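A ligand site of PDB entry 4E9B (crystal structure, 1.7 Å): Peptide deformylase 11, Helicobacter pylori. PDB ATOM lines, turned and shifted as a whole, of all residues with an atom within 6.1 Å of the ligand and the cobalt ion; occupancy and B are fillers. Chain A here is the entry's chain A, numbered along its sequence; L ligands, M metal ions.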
ATOM      1  N   SER A  41      30.894  15.123  30.712  1.00  0.00           N
ATOM      2  CA  SER A  41      29.689  15.082  29.891  1.00  0.00           C
ATOM      3  C   SER A  41      28.442  14.485  30.556  1.00  0.00           C
ATOM      4  O   SER A  41      27.399  14.427  29.924  1.00  0.00           O
ATOM      5  CB  SER A  41      29.985  14.315  28.598  1.00  0.00           C
ATOM      6  OG  SER A  41      30.548  15.199  27.659  1.00  0.00           O
ATOM      7  N   GLU A  42      28.558  14.050  31.806  1.00  0.00           N
ATOM      8  CA  GLU A  42      27.488  13.484  32.631  1.00  0.00           C
ATOM      9  C   GLU A  42      26.914  12.218  31.991  1.00  0.00           C
ATOM     10  O   GLU A  42      25.702  11.972  31.985  1.00  0.00           O
ATOM     11  CB  GLU A  42      26.423  14.553  32.975  1.00  0.00           C
ATOM     12  CG  GLU A  42      27.083  15.780  33.638  1.00  0.00           C
ATOM     13  CD  GLU A  42      26.166  16.985  33.807  1.00  0.00           C
ATOM     14  OE1 GLU A  42      24.925  16.811  33.846  1.00  0.00           O
ATOM     15  OE2 GLU A  42      26.703  18.126  33.903  1.00  0.00           O
ATOM     16  N   GLY A  43      27.819  11.407  31.437  1.00  0.00           N
ATOM     17  CA  GLY A  43      27.428  10.081  30.952  1.00  0.00           C
ATOM     18  C   GLY A  43      27.678   9.048  32.030  1.00  0.00           C
ATOM     19  O   GLY A  43      28.370   9.306  33.025  1.00  0.00           O
ATOM     20  N   ILE A  44      27.104   7.871  31.834  1.00  0.00           N
ATOM     21  CA  ILE A  44      27.382   6.743  32.726  1.00  0.00           C
ATOM     22  C   ILE A  44      28.190   5.662  32.027  1.00  0.00           C
ATOM     23  O   ILE A  44      28.514   4.646  32.649  1.00  0.00           O
ATOM     24  CB  ILE A  44      26.104   6.130  33.323  1.00  0.00           C
ATOM     25  CG1 ILE A  44      25.160   5.607  32.225  1.00  0.00           C
ATOM     26  CG2 ILE A  44      25.394   7.189  34.174  1.00  0.00           C
ATOM     27  CD1 ILE A  44      24.023   4.715  32.761  1.00  0.00           C
ATOM     28  N   GLY A  45      28.480   5.882  30.752  1.00  0.00           N
ATOM     29  CA  GLY A  45      29.381   4.984  30.054  1.00  0.00           C
ATOM     30  C   GLY A  45      30.016   5.765  28.926  1.00  0.00           C
ATOM     31  O   GLY A  45      29.589   6.870  28.596  1.00  0.00           O
ATOM     32  N   LEU A  46      31.039   5.178  28.322  1.00  0.00           N
ATOM     33  CA  LEU A  46      31.632   5.764  27.109  1.00  0.00           C
ATOM     34  C   LEU A  46      32.422   4.701  26.363  1.00  0.00           C
ATOM     35  O   LEU A  46      33.133   3.932  26.997  1.00  0.00           O
ATOM     36  CB  LEU A  46      32.596   6.929  27.478  1.00  0.00           C
ATOM     37  CG  LEU A  46      33.051   7.817  26.306  1.00  0.00           C
ATOM     38  CD1 LEU A  46      31.916   8.657  25.744  1.00  0.00           C
ATOM     39  CD2 LEU A  46      34.184   8.711  26.793  1.00  0.00           C
ATOM     40  N   ALA A  47      32.312   4.673  25.035  1.00  0.00           N
ATOM     41  CA  ALA A  47      33.081   3.735  24.194  1.00  0.00           C
ATOM     42  C   ALA A  47      34.200   4.524  23.545  1.00  0.00           C
ATOM     43  O   ALA A  47      34.039   5.717  23.210  1.00  0.00           O
ATOM     44  CB  ALA A  47      32.167   3.115  23.121  1.00  0.00           C
ATOM     45  N   GLN A  50      33.670   6.830  20.488  1.00  0.00           N
ATOM     46  CA  GLN A  50      32.998   8.102  20.733  1.00  0.00           C
ATOM     47  C   GLN A  50      33.977   9.283  20.900  1.00  0.00           C
ATOM     48  O   GLN A  50      33.565  10.445  20.742  1.00  0.00           O
ATOM     49  CB  GLN A  50      32.065   8.001  21.947  1.00  0.00           C
ATOM     50  CG  GLN A  50      30.899   7.053  21.691  1.00  0.00           C
ATOM     51  CD  GLN A  50      30.010   6.976  22.893  1.00  0.00           C
ATOM     52  OE1 GLN A  50      30.234   6.184  23.831  1.00  0.00           O
ATOM     53  NE2 GLN A  50      28.994   7.848  22.916  1.00  0.00           N
ATOM     54  N   TYR A  91      14.263  -0.352  27.657  1.00  0.00           N
ATOM     55  CA  TYR A  91      14.906   0.642  28.473  1.00  0.00           C
ATOM     56  C   TYR A  91      14.990   1.943  27.673  1.00  0.00           C
ATOM     57  O   TYR A  91      15.331   1.901  26.495  1.00  0.00           O
ATOM     58  CB  TYR A  91      16.306   0.157  28.920  1.00  0.00           C
ATOM     59  CG  TYR A  91      16.719   0.785  30.219  1.00  0.00           C
ATOM     60  CD1 TYR A  91      16.525   0.118  31.421  1.00  0.00           C
ATOM     61  CD2 TYR A  91      17.263   2.068  30.239  1.00  0.00           C
ATOM     62  CE1 TYR A  91      16.883   0.704  32.632  1.00  0.00           C
ATOM     63  CE2 TYR A  91      17.617   2.664  31.441  1.00  0.00           C
ATOM     64  CZ  TYR A  91      17.415   1.985  32.623  1.00  0.00           C
ATOM     65  OH  TYR A  91      17.771   2.572  33.804  1.00  0.00           O
ATOM     66  N   LYS A  92      14.697   3.072  28.318  1.00  0.00           N
ATOM     67  CA  LYS A  92      14.796   4.389  27.678  1.00  0.00           C
ATOM     68  C   LYS A  92      16.248   4.858  27.746  1.00  0.00           C
ATOM     69  O   LYS A  92      16.818   4.982  28.825  1.00  0.00           O
ATOM     70  CB  LYS A  92      13.906   5.402  28.430  1.00  0.00           C
ATOM     71  CG  LYS A  92      13.671   6.740  27.724  1.00  0.00           C
ATOM     72  CD  LYS A  92      12.574   6.608  26.672  1.00  0.00           C
ATOM     73  CE  LYS A  92      11.961   7.936  26.242  1.00  0.00           C
ATOM     74  NZ  LYS A  92      10.525   8.030  26.616  1.00  0.00           N
ATOM     75  N   GLU A  93      16.853   5.058  26.589  1.00  0.00           N
ATOM     76  CA  GLU A  93      18.263   5.398  26.514  1.00  0.00           C
ATOM     77  C   GLU A  93      18.445   6.701  25.798  1.00  0.00           C
ATOM     78  O   GLU A  93      17.647   7.042  24.923  1.00  0.00           O
ATOM     79  CB  GLU A  93      19.015   4.340  25.680  1.00  0.00           C
ATOM     80  CG  GLU A  93      18.942   2.960  26.275  1.00  0.00           C
ATOM     81  CD  GLU A  93      19.687   1.930  25.453  1.00  0.00           C
ATOM     82  OE1 GLU A  93      20.679   2.289  24.756  1.00  0.00           O
ATOM     83  OE2 GLU A  93      19.280   0.766  25.507  1.00  0.00           O
ATOM     84  N   GLY A  94      19.541   7.374  26.149  1.00  0.00           N
ATOM     85  CA  GLY A  94      20.098   8.407  25.317  1.00  0.00           C
ATOM     86  C   GLY A  94      21.547   8.047  25.093  1.00  0.00           C
ATOM     87  O   GLY A  94      22.068   7.060  25.662  1.00  0.00           O
ATOM     88  N   CYS A  95      22.210   8.869  24.296  1.00  0.00           N
ATOM     89  CA  CYS A  95      23.610   8.609  23.908  1.00  0.00           C
ATOM     90  C   CYS A  95      24.355   9.926  23.796  1.00  0.00           C
ATOM     91  O   CYS A  95      23.831  10.883  23.196  1.00  0.00           O
ATOM     92  CB  CYS A  95      23.631   7.879  22.565  1.00  0.00           C
ATOM     93  SG  CYS A  95      25.287   7.479  21.914  1.00  0.00           S
ATOM     94  N   LEU A  96      25.590   9.982  24.325  1.00  0.00           N
ATOM     95  CA  LEU A  96      26.407  11.196  24.204  1.00  0.00           C
ATOM     96  C   LEU A  96      26.710  11.545  22.731  1.00  0.00           C
ATOM     97  O   LEU A  96      26.975  12.714  22.416  1.00  0.00           O
ATOM     98  CB  LEU A  96      27.706  11.088  25.003  1.00  0.00           C
ATOM     99  CG  LEU A  96      27.503  10.941  26.526  1.00  0.00           C
ATOM    100  CD1 LEU A  96      28.876  10.761  27.146  1.00  0.00           C
ATOM    101  CD2 LEU A  96      26.861  12.206  27.049  1.00  0.00           C
ATOM    102  N   SER A  97      26.676  10.555  21.834  1.00  0.00           N
ATOM    103  CA  SER A  97      26.877  10.799  20.415  1.00  0.00           C
ATOM    104  C   SER A  97      25.596  11.171  19.644  1.00  0.00           C
ATOM    105  O   SER A  97      25.643  11.492  18.470  1.00  0.00           O
ATOM    106  CB  SER A  97      27.558   9.587  19.730  1.00  0.00           C
ATOM    107  OG  SER A  97      28.863   9.443  20.277  1.00  0.00           O
ATOM    108  N   TYR A 102      16.002  10.638  23.186  1.00  0.00           N
ATOM    109  CA  TYR A 102      15.802   9.506  24.100  1.00  0.00           C
ATOM    110  C   TYR A 102      14.672   8.666  23.585  1.00  0.00           C
ATOM    111  O   TYR A 102      13.617   9.205  23.227  1.00  0.00           O
ATOM    112  CB  TYR A 102      15.465   9.973  25.515  1.00  0.00           C
ATOM    113  CG  TYR A 102      16.445  11.001  25.998  1.00  0.00           C
ATOM    114  CD1 TYR A 102      16.223  12.348  25.743  1.00  0.00           C
ATOM    115  CD2 TYR A 102      17.622  10.637  26.645  1.00  0.00           C
ATOM    116  CE1 TYR A 102      17.146  13.302  26.146  1.00  0.00           C
ATOM    117  CE2 TYR A 102      18.539  11.578  27.058  1.00  0.00           C
ATOM    118  CZ  TYR A 102      18.281  12.905  26.795  1.00  0.00           C
ATOM    119  OH  TYR A 102      19.179  13.872  27.191  1.00  0.00           O
ATOM    120  N   LEU A 130      20.017  -1.967  34.482  1.00  0.00           N
ATOM    121  CA  LEU A 130      20.774  -0.858  33.889  1.00  0.00           C
ATOM    122  C   LEU A 130      22.186  -1.262  33.516  1.00  0.00           C
ATOM    123  O   LEU A 130      22.702  -0.843  32.463  1.00  0.00           O
ATOM    124  CB  LEU A 130      20.832   0.312  34.862  1.00  0.00           C
ATOM    125  CG  LEU A 130      21.605   1.525  34.343  1.00  0.00           C
ATOM    126  CD1 LEU A 130      21.101   1.979  32.980  1.00  0.00           C
ATOM    127  CD2 LEU A 130      21.501   2.623  35.394  1.00  0.00           C
ATOM    128  N   VAL A 133      22.076  -3.090  30.305  1.00  0.00           N
ATOM    129  CA  VAL A 133      21.737  -2.186  29.199  1.00  0.00           C
ATOM    130  C   VAL A 133      22.961  -1.350  28.804  1.00  0.00           C
ATOM    131  O   VAL A 133      23.255  -1.197  27.626  1.00  0.00           O
ATOM    132  CB  VAL A 133      20.557  -1.257  29.576  1.00  0.00           C
ATOM    133  CG1 VAL A 133      20.318  -0.230  28.477  1.00  0.00           C
ATOM    134  CG2 VAL A 133      19.315  -2.099  29.811  1.00  0.00           C
ATOM    135  N   ALA A 134      23.651  -0.833  29.810  1.00  0.00           N
ATOM    136  CA  ALA A 134      24.849  -0.023  29.557  1.00  0.00           C
ATOM    137  C   ALA A 134      25.906  -0.852  28.820  1.00  0.00           C
ATOM    138  O   ALA A 134      26.489  -0.398  27.854  1.00  0.00           O
ATOM    139  CB  ALA A 134      25.419   0.536  30.862  1.00  0.00           C
ATOM    140  N   HIS A 137      24.706  -1.179  25.200  1.00  0.00           N
ATOM    141  CA  HIS A 137      24.846   0.091  24.496  1.00  0.00           C
ATOM    142  C   HIS A 137      26.302   0.316  24.112  1.00  0.00           C
ATOM    143  O   HIS A 137      26.624   0.663  22.960  1.00  0.00           O
ATOM    144  CB  HIS A 137      24.309   1.176  25.406  1.00  0.00           C
ATOM    145  CG  HIS A 137      24.403   2.560  24.840  1.00  0.00           C
ATOM    146  ND1 HIS A 137      23.290   3.267  24.522  1.00  0.00           N
ATOM    147  CD2 HIS A 137      25.483   3.387  24.596  1.00  0.00           C
ATOM    148  CE1 HIS A 137      23.649   4.482  24.071  1.00  0.00           C
ATOM    149  NE2 HIS A 137      24.996   4.557  24.101  1.00  0.00           N
ATOM    150  N   GLU A 138      27.217   0.121  25.045  1.00  0.00           N
ATOM    151  CA  GLU A 138      28.630   0.402  24.737  1.00  0.00           C
ATOM    152  C   GLU A 138      29.213  -0.604  23.767  1.00  0.00           C
ATOM    153  O   GLU A 138      30.001  -0.222  22.904  1.00  0.00           O
ATOM    154  CB  GLU A 138      29.491   0.422  26.003  1.00  0.00           C
ATOM    155  CG  GLU A 138      29.009   1.388  27.075  1.00  0.00           C
ATOM    156  CD  GLU A 138      28.953   2.814  26.652  1.00  0.00           C
ATOM    157  OE1 GLU A 138      29.588   3.151  25.627  1.00  0.00           O
ATOM    158  OE2 GLU A 138      28.276   3.621  27.340  1.00  0.00           O
ATOM    159  N   HIS A 141      28.386   0.317  20.277  1.00  0.00           N
ATOM    160  CA  HIS A 141      29.325   1.309  19.718  1.00  0.00           C
ATOM    161  C   HIS A 141      30.565   0.669  19.147  1.00  0.00           C
ATOM    162  O   HIS A 141      31.074   1.156  18.147  1.00  0.00           O
ATOM    163  CB  HIS A 141      29.782   2.309  20.767  1.00  0.00           C
ATOM    164  CG  HIS A 141      28.804   3.419  21.027  1.00  0.00           C
ATOM    165  ND1 HIS A 141      28.394   4.273  20.064  1.00  0.00           N
ATOM    166  CD2 HIS A 141      28.218   3.837  22.217  1.00  0.00           C
ATOM    167  CE1 HIS A 141      27.536   5.171  20.609  1.00  0.00           C
ATOM    168  NE2 HIS A 141      27.424   4.886  21.920  1.00  0.00           N
ATOM    169  N   LEU A 146      24.482   2.506  16.757  1.00  0.00           N
ATOM    170  CA  LEU A 146      23.890   3.525  17.629  1.00  0.00           C
ATOM    171  C   LEU A 146      22.501   3.069  18.019  1.00  0.00           C
ATOM    172  O   LEU A 146      21.850   2.330  17.273  1.00  0.00           O
ATOM    173  CB  LEU A 146      23.776   4.870  16.885  1.00  0.00           C
ATOM    174  CG  LEU A 146      25.111   5.412  16.362  1.00  0.00           C
ATOM    175  CD1 LEU A 146      24.879   6.684  15.553  1.00  0.00           C
ATOM    176  CD2 LEU A 146      26.031   5.673  17.542  1.00  0.00           C
ATOM    177  N   PHE A 147      22.017   3.529  19.183  1.00  0.00           N
ATOM    178  CA  PHE A 147      20.745   2.977  19.661  1.00  0.00           C
ATOM    179  C   PHE A 147      19.609   3.350  18.700  1.00  0.00           C
ATOM    180  O   PHE A 147      18.606   2.626  18.622  1.00  0.00           O
ATOM    181  CB  PHE A 147      20.423   3.404  21.124  1.00  0.00           C
ATOM    182  CG  PHE A 147      19.914   4.813  21.262  1.00  0.00           C
ATOM    183  CD1 PHE A 147      20.798   5.893  21.262  1.00  0.00           C
ATOM    184  CD2 PHE A 147      18.543   5.065  21.386  1.00  0.00           C
ATOM    185  CE1 PHE A 147      20.329   7.199  21.394  1.00  0.00           C
ATOM    186  CE2 PHE A 147      18.076   6.362  21.518  1.00  0.00           C
ATOM    187  CZ  PHE A 147      18.953   7.429  21.517  1.00  0.00           C
HETATM  188  C1  LIG L   1      26.467   7.349  27.385  1.00  0.00           C
HETATM  189  C2  LIG L   1      26.917   6.859  26.021  1.00  0.00           C
HETATM  190  O1  LIG L   1      26.545   7.426  24.995  1.00  0.00           O
HETATM  191  N1  LIG L   1      27.716   5.800  25.987  1.00  0.00           N
HETATM  192  O2  LIG L   1      27.926   5.257  24.698  1.00  0.00           O
HETATM  193  C3  LIG L   1      25.126   6.721  27.735  1.00  0.00           C
HETATM  194  C4  LIG L   1      24.486   7.581  28.774  1.00  0.00           C
HETATM  195  O3  LIG L   1      25.113   7.947  29.748  1.00  0.00           O
HETATM  196  C5  LIG L   1      25.367   5.347  28.369  1.00  0.00           C
HETATM  197  C6  LIG L   1      24.115   4.671  28.911  1.00  0.00           C
HETATM  198  C7  LIG L   1      23.392   3.866  27.858  1.00  0.00           C
HETATM  199  C8  LIG L   1      22.297   2.942  28.430  1.00  0.00           C
HETATM  200  C9  LIG L   1      21.288   3.641  29.318  1.00  0.00           C
HETATM  201  N2  LIG L   1      23.232   7.930  28.533  1.00  0.00           N
HETATM  202  C10 LIG L   1      22.387   8.588  29.519  1.00  0.00           C
HETATM  203  C11 LIG L   1      22.032   9.976  28.974  1.00  0.00           C
HETATM  204  C12 LIG L   1      21.057  10.705  29.881  1.00  0.00           C
HETATM  205  C13 LIG L   1      23.273  10.819  28.729  1.00  0.00           C
HETATM  206  C14 LIG L   1      21.160   7.753  29.703  1.00  0.00           C
HETATM  207  O4  LIG L   1      20.610   7.296  28.710  1.00  0.00           O
HETATM  208  N3  LIG L   1      20.722   7.461  30.936  1.00  0.00           N
HETATM  209  C15 LIG L   1      19.579   6.548  31.081  1.00  0.00           C
HETATM  210  C16 LIG L   1      21.300   7.879  32.205  1.00  0.00           C
HETATM  211  C17 LIG L   1      20.569   7.054  33.258  1.00  0.00           C
HETATM  212  C18 LIG L   1      19.688   6.069  32.520  1.00  0.00           C
HETATM  213  C19 LIG L   1      18.295   7.357  30.849  1.00  0.00           C
HETATM  214  O5  LIG L   1      17.168   6.476  31.074  1.00  0.00           O
HETATM  215 CO    CO M   1      26.369   5.998  23.379  1.00  0.00          CO
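OE2 of Glu 138 is in hydrogen-bond range of N1 of the ligand, at 2.6 Å. OE1 of Gln 50 sits at hydrogen-bond distance from N1 of the ligand, 3.3 Å away. An oxygen (O5) of the ligand sits at hydrogen-bond distance from the backbone carbonyl oxygen (O) of Lys 92 (2.7 Å). N of Gly 94 is in hydrogen-bond range of O4 of the ligand. The backbone carbonyl oxygen of Gly 94 lies within hydrogen-bond range of a nitrogen (N2) of the ligand (3.2 Å). An oxygen (O1) of the ligand lies close to the backbone NH of Leu 96 (2.8 Å). An oxygen (O3) of the ligand is in hydrogen-bond range of the backbone NH (N) of Ile 44. The backbone carbonyl oxygen (O) of Gly 45 lies close to a nitrogen (N1) of the ligand, 3.4 Å away.
NE2 of Gln 50 lies close to NE2 of His 141. ND1 of His 137 lies within hydrogen-bond range of OE1 of Glu 93 (2.8 Å). The backbone NH (N) of Ser 97 sits close to the side-chain sulfur (SG) of Cys 95, 3.4 Å away. OE2 of Glu 138 sits at hydrogen-bond distance from N of Leu 46, at 3.3 Å. The backbone NH of Ala 47 is in hydrogen-bond range of the side-chain carboxylate of Glu 138 (3.2 Å). N of Ala 47 sits at hydrogen-bond distance from OE1 of Gln 50 (2.8 Å). The side-chain amide nitrogen of Gln 50 sits at hydrogen-bond distance from the side-chain hydroxyl of Ser 97.
Gly 43 touches the ligand (CA to O3, 3.4 Å). Tyr 91 touches the ligand. Glu 93 touches the ligand (C to O4, 3.7 Å). Tyr 102 touches the ligand. CG1 of Val 133 touches C8 of the ligand, at 3.7 Å. Hydrophobic or aromatic side chains that line the ligand: Ile 44, Tyr 91, Leu 96, Tyr 102, Val 133, His 137 and His 141. Within 4 Å of the ligand: Gly 43, Ile 44, Gly 45, Gln 50, Tyr 91, Lys 92, Glu 93, Gly 94, Cys 95, Leu 96, Tyr 102, Val 133, His 137, Glu 138 and His 141.
Gln 50 touches the cobalt ion (NE2 to CO, 3.2 Å). Along chain A the residues within 4 Å of the cobalt ion span positions 50 to 141. The nearest printed residue that does not touch the cobalt ion is Leu 96 (4.2 Å).
The cobalt ion is bound by a ring nitrogen (NE2) of His 141, a ring nitrogen (NE2) of His 137, an oxygen (O1) of the ligand, an oxygen (O2) of the ligand and the side-chain sulfur (SG) of Cys 95.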
